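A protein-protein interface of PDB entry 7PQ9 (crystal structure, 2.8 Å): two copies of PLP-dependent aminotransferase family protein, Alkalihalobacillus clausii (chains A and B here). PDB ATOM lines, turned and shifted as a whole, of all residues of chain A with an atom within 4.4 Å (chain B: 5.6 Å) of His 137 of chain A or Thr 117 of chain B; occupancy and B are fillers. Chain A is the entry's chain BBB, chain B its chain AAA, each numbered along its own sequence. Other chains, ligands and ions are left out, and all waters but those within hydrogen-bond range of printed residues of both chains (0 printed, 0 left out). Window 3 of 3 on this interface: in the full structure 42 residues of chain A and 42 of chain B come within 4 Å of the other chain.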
ATOM      1  N   CYS A 133      -9.587 -10.847  -8.248  1.00  0.00           N
ATOM      2  CA  CYS A 133     -10.334 -10.423  -7.065  1.00  0.00           C
ATOM      3  C   CYS A 133      -9.380 -10.027  -5.925  1.00  0.00           C
ATOM      4  O   CYS A 133      -8.207 -10.402  -5.928  1.00  0.00           O
ATOM      5  CB  CYS A 133     -11.181 -11.581  -6.577  1.00  0.00           C
ATOM      6  SG  CYS A 133     -10.194 -12.907  -5.834  1.00  0.00           S
ATOM      7  N   LYS A 134      -9.914  -9.294  -4.941  1.00  0.00           N
ATOM      8  CA  LYS A 134      -9.130  -8.601  -3.924  1.00  0.00           C
ATOM      9  C   LYS A 134      -8.165  -9.546  -3.189  1.00  0.00           C
ATOM     10  O   LYS A 134      -7.062  -9.143  -2.820  1.00  0.00           O
ATOM     11  CB  LYS A 134     -10.060  -7.770  -3.026  1.00  0.00           C
ATOM     12  CG  LYS A 134      -9.468  -7.250  -1.721  1.00  0.00           C
ATOM     13  CD  LYS A 134      -9.561  -5.755  -1.454  1.00  0.00           C
ATOM     14  CE  LYS A 134      -8.554  -5.330  -0.405  1.00  0.00           C
ATOM     15  NZ  LYS A 134      -9.185  -4.417   0.575  1.00  0.00           N
ATOM     16  N   GLU A 135      -8.557 -10.808  -2.996  1.00  0.00           N
ATOM     17  CA  GLU A 135      -7.765 -11.754  -2.216  1.00  0.00           C
ATOM     18  C   GLU A 135      -6.505 -12.154  -2.982  1.00  0.00           C
ATOM     19  O   GLU A 135      -5.462 -12.396  -2.384  1.00  0.00           O
ATOM     20  CB  GLU A 135      -8.547 -12.953  -1.667  1.00  0.00           C
ATOM     21  CG  GLU A 135      -9.711 -13.503  -2.488  1.00  0.00           C
ATOM     22  CD  GLU A 135     -11.056 -12.797  -2.320  1.00  0.00           C
ATOM     23  OE1 GLU A 135     -11.186 -11.624  -2.709  1.00  0.00           O
ATOM     24  OE2 GLU A 135     -11.982 -13.431  -1.801  1.00  0.00           O
ATOM     25  N   ASN A 136      -6.595 -12.154  -4.311  1.00  0.00           N
ATOM     26  CA  ASN A 136      -5.478 -12.519  -5.172  1.00  0.00           C
ATOM     27  C   ASN A 136      -4.721 -11.288  -5.667  1.00  0.00           C
ATOM     28  O   ASN A 136      -4.091 -11.319  -6.729  1.00  0.00           O
ATOM     29  CB  ASN A 136      -5.985 -13.267  -6.397  1.00  0.00           C
ATOM     30  CG  ASN A 136      -6.453 -14.642  -6.005  1.00  0.00           C
ATOM     31  OD1 ASN A 136      -5.931 -15.210  -5.055  1.00  0.00           O
ATOM     32  ND2 ASN A 136      -7.432 -15.173  -6.717  1.00  0.00           N
ATOM     33  N   HIS A 137      -4.760 -10.207  -4.875  1.00  0.00           N
ATOM     34  CA  HIS A 137      -4.236  -8.942  -5.332  1.00  0.00           C
ATOM     35  C   HIS A 137      -2.769  -9.062  -5.755  1.00  0.00           C
ATOM     36  O   HIS A 137      -2.298  -8.282  -6.578  1.00  0.00           O
ATOM     37  CB  HIS A 137      -4.494  -7.865  -4.291  1.00  0.00           C
ATOM     38  CG  HIS A 137      -3.706  -8.022  -3.045  1.00  0.00           C
ATOM     39  ND1 HIS A 137      -2.441  -7.459  -2.892  1.00  0.00           N
ATOM     40  CD2 HIS A 137      -3.988  -8.656  -1.903  1.00  0.00           C
ATOM     41  CE1 HIS A 137      -1.987  -7.693  -1.685  1.00  0.00           C
ATOM     42  NE2 HIS A 137      -2.929  -8.396  -1.041  1.00  0.00           N
ATOM     43  N   ARG A 138      -2.056 -10.045  -5.210  1.00  0.00           N
ATOM     44  CA  ARG A 138      -0.631 -10.153  -5.481  1.00  0.00           C
ATOM     45  C   ARG A 138      -0.389 -10.626  -6.915  1.00  0.00           C
ATOM     46  O   ARG A 138       0.686 -10.396  -7.470  1.00  0.00           O
ATOM     47  CB  ARG A 138       0.078 -10.979  -4.400  1.00  0.00           C
ATOM     48  CG  ARG A 138       0.482 -10.187  -3.160  1.00  0.00           C
ATOM     49  CD  ARG A 138       0.376 -11.015  -1.878  1.00  0.00           C
ATOM     50  NE  ARG A 138       1.261 -10.576  -0.799  1.00  0.00           N
ATOM     51  CZ  ARG A 138       2.343 -11.233  -0.360  1.00  0.00           C
ATOM     52  NH1 ARG A 138       3.066 -10.731   0.629  1.00  0.00           N
ATOM     53  NH2 ARG A 138       2.697 -12.393  -0.895  1.00  0.00           N
ATOM     54  N   LEU A 139      -1.415 -11.225  -7.540  1.00  0.00           N
ATOM     55  CA  LEU A 139      -1.344 -11.666  -8.928  1.00  0.00           C
ATOM     56  C   LEU A 139      -1.117 -10.492  -9.876  1.00  0.00           C
ATOM     57  O   LEU A 139      -0.691 -10.694 -11.003  1.00  0.00           O
ATOM     58  CB  LEU A 139      -2.631 -12.409  -9.299  1.00  0.00           C
ATOM     59  CG  LEU A 139      -2.747 -13.811  -8.684  1.00  0.00           C
ATOM     60  CD1 LEU A 139      -3.902 -14.598  -9.308  1.00  0.00           C
ATOM     61  CD2 LEU A 139      -1.432 -14.589  -8.794  1.00  0.00           C
ATOM     62  N   LEU A 140      -1.405  -9.265  -9.424  1.00  0.00           N
ATOM     63  CA  LEU A 140      -1.233  -8.082 -10.255  1.00  0.00           C
ATOM     64  C   LEU A 140       0.244  -7.741 -10.432  1.00  0.00           C
ATOM     65  O   LEU A 140       0.587  -7.064 -11.397  1.00  0.00           O
ATOM     66  CB  LEU A 140      -2.014  -6.896  -9.676  1.00  0.00           C
ATOM     67  CG  LEU A 140      -3.519  -7.124  -9.461  1.00  0.00           C
ATOM     68  CD1 LEU A 140      -4.227  -5.824  -9.183  1.00  0.00           C
ATOM     69  CD2 LEU A 140      -4.202  -7.830 -10.648  1.00  0.00           C
ATOM     70  N   ASP B 115       0.048  -0.325  -5.936  1.00  0.00           N
ATOM     71  CA  ASP B 115      -0.852  -0.633  -4.846  1.00  0.00           C
ATOM     72  C   ASP B 115      -1.906  -1.617  -5.322  1.00  0.00           C
ATOM     73  O   ASP B 115      -2.924  -1.208  -5.852  1.00  0.00           O
ATOM     74  CB  ASP B 115      -1.415   0.608  -4.161  1.00  0.00           C
ATOM     75  CG  ASP B 115      -2.130   0.233  -2.868  1.00  0.00           C
ATOM     76  OD1 ASP B 115      -2.972  -0.683  -2.895  1.00  0.00           O
ATOM     77  OD2 ASP B 115      -1.815   0.844  -1.837  1.00  0.00           O
ATOM     78  N   THR B 116      -1.661  -2.906  -5.084  1.00  0.00           N
ATOM     79  CA  THR B 116      -2.496  -3.966  -5.618  1.00  0.00           C
ATOM     80  C   THR B 116      -3.859  -3.994  -4.942  1.00  0.00           C
ATOM     81  O   THR B 116      -4.843  -4.374  -5.571  1.00  0.00           O
ATOM     82  CB  THR B 116      -1.786  -5.316  -5.528  1.00  0.00           C
ATOM     83  OG1 THR B 116      -1.299  -5.392  -4.181  1.00  0.00           O
ATOM     84  CG2 THR B 116      -0.704  -5.434  -6.580  1.00  0.00           C
ATOM     85  N   THR B 117      -3.911  -3.593  -3.671  1.00  0.00           N
ATOM     86  CA  THR B 117      -5.137  -3.697  -2.875  1.00  0.00           C
ATOM     87  C   THR B 117      -6.192  -2.701  -3.381  1.00  0.00           C
ATOM     88  O   THR B 117      -7.388  -2.946  -3.270  1.00  0.00           O
ATOM     89  CB  THR B 117      -4.813  -3.573  -1.383  1.00  0.00           C
ATOM     90  OG1 THR B 117      -4.485  -2.204  -1.163  1.00  0.00           O
ATOM     91  CG2 THR B 117      -3.595  -4.371  -0.967  1.00  0.00           C
ATOM     92  N   SER B 118      -5.720  -1.607  -3.993  1.00  0.00           N
ATOM     93  CA  SER B 118      -6.499  -0.454  -4.445  1.00  0.00           C
ATOM     94  C   SER B 118      -7.160  -0.676  -5.802  1.00  0.00           C
ATOM     95  O   SER B 118      -7.940   0.162  -6.244  1.00  0.00           O
ATOM     96  CB  SER B 118      -5.628   0.782  -4.557  1.00  0.00           C
ATOM     97  OG  SER B 118      -4.783   0.909  -3.426  1.00  0.00           O
ATOM     98  N   PHE B 119      -6.854  -1.764  -6.492  1.00  0.00           N
ATOM     99  CA  PHE B 119      -7.199  -1.847  -7.898  1.00  0.00           C
ATOM    100  C   PHE B 119      -8.713  -2.042  -8.040  1.00  0.00           C
ATOM    101  O   PHE B 119      -9.322  -2.782  -7.266  1.00  0.00           O
ATOM    102  CB  PHE B 119      -6.398  -2.966  -8.591  1.00  0.00           C
ATOM    103  CG  PHE B 119      -6.666  -3.043 -10.071  1.00  0.00           C
ATOM    104  CD1 PHE B 119      -5.945  -2.260 -10.971  1.00  0.00           C
ATOM    105  CD2 PHE B 119      -7.677  -3.846 -10.571  1.00  0.00           C
ATOM    106  CE1 PHE B 119      -6.234  -2.265 -12.338  1.00  0.00           C
ATOM    107  CE2 PHE B 119      -7.949  -3.886 -11.938  1.00  0.00           C
ATOM    108  CZ  PHE B 119      -7.233  -3.095 -12.818  1.00  0.00           C
ATOM    109  N   PHE B 121     -11.063  -4.031  -8.948  1.00  0.00           N
ATOM    110  CA  PHE B 121     -11.399  -5.399  -9.328  1.00  0.00           C
ATOM    111  C   PHE B 121     -12.805  -5.496  -9.900  1.00  0.00           C
ATOM    112  O   PHE B 121     -13.017  -6.240 -10.869  1.00  0.00           O
ATOM    113  CB  PHE B 121     -11.213  -6.370  -8.164  1.00  0.00           C
ATOM    114  CG  PHE B 121      -9.801  -6.440  -7.652  1.00  0.00           C
ATOM    115  CD1 PHE B 121      -8.847  -7.235  -8.283  1.00  0.00           C
ATOM    116  CD2 PHE B 121      -9.409  -5.664  -6.575  1.00  0.00           C
ATOM    117  CE1 PHE B 121      -7.543  -7.287  -7.811  1.00  0.00           C
ATOM    118  CE2 PHE B 121      -8.101  -5.702  -6.113  1.00  0.00           C
ATOM    119  CZ  PHE B 121      -7.172  -6.519  -6.729  1.00  0.00           C
ATOM    120  N   PRO B 447       1.215  -1.464   2.008  1.00  0.00           N
ATOM    121  CA  PRO B 447      -0.133  -0.928   2.219  1.00  0.00           C
ATOM    122  C   PRO B 447      -0.053   0.349   3.054  1.00  0.00           C
ATOM    123  O   PRO B 447       0.856   0.505   3.890  1.00  0.00           O
ATOM    124  CB  PRO B 447      -0.892  -2.073   2.904  1.00  0.00           C
ATOM    125  CG  PRO B 447      -0.012  -3.294   2.730  1.00  0.00           C
ATOM    126  CD  PRO B 447       1.413  -2.765   2.668  1.00  0.00           C
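Of chain A, only Lys 134 (3.9 Å) and His 137 (3.8 Å) come within 4 Å of Thr 117 of chain B.
Printed residues of chain A within 4 Å of Phe 119 of chain B: Leu 140.
Printed residues of chain B within 4 Å of Cys 133 of chain A: Phe 121 (3.7 Å).
Printed residues of chain B within 4 Å of Lys 134 of chain A: Thr 117 and Phe 121.
Of the printed residues of chain B, Leu 140 of chain A touches Thr 116 (3.7 Å), Phe 119 (3.6 Å) and Phe 121 (3.9 Å).
Ser 118 of chain B touches none of the printed residues of chain A.
Pro 447 of chain B touches none of the printed residues of chain A.
The nearest printed residue of chain B that does not touch His 137 of chain A is Asp 115 of chain B (6.3 Å).
The nearest printed residue of chain A that does not touch Thr 117 of chain B is Leu 140 of chain A (6.0 Å).
The nearest printed residue of chain A that does not touch Phe 121 of chain B is Asn 136 of chain A (5.3 Å).
The side-chain hydroxyl (OG1) of Thr 116 of chain B sits at hydrogen-bond distance from a ring nitrogen (ND1) of His 137 of chain A (2.7 Å).
No position is printed for both chains.
Of the 9 pairs that touch across the chains among the printed residues, none has its exchanged pair printed and touching as well.
SG of Cys 133 of chain A is in hydrogen-bond range of ND2 of Asn 136 of chain A, at 3.7 Å.
The side-chain carboxylate (OD1) of Asp 115 of chain B is in hydrogen-bond range of the side-chain hydroxyl (OG1) of Thr 117 of chain B, at 2.8 Å.
The side-chain sulfur of Cys 133 of chain A sits close to the side-chain carboxylate of Glu 135 of chain A, at 3.5 Å.
Of the 7 printed residues of chain B, 4 touch a printed residue of chain A.
Hydrophobic or aromatic side chains of chain B that line the printed part of chain A: Phe 119 and Phe 121.
Hydrophobic or aromatic side chains of chain A within 4 Å of the printed part of chain B: His 137 and Leu 140.
Along chain A the printed residues that touch a printed residue of chain B span positions 133 to 140.
Among the printed residues, 9 pairs touch across the chains.
Among the printed residues, no Asp or Glu carboxylate lies within 4 Å of a Lys or Arg side-chain nitrogen of the other chain.
N of Cys 133 of chain A touches CD1 of Phe 121 of chain B, 3.7 Å away.
Lys 134 of chain A touches Thr 117 of chain B.
Lys 134 of chain A touches Phe 121 of chain B.
His 137 of chain A touches Thr 117 of chain B.
Phe 121 of chain B touches His 137 of chain A.
Thr 116 of chain B touches Leu 140 of chain A.
Leu 140 of chain A touches Phe 119 of chain B.
Leu 140 of chain A touches Phe 121 of chain B (CD1 to CE1, 3.9 Å).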
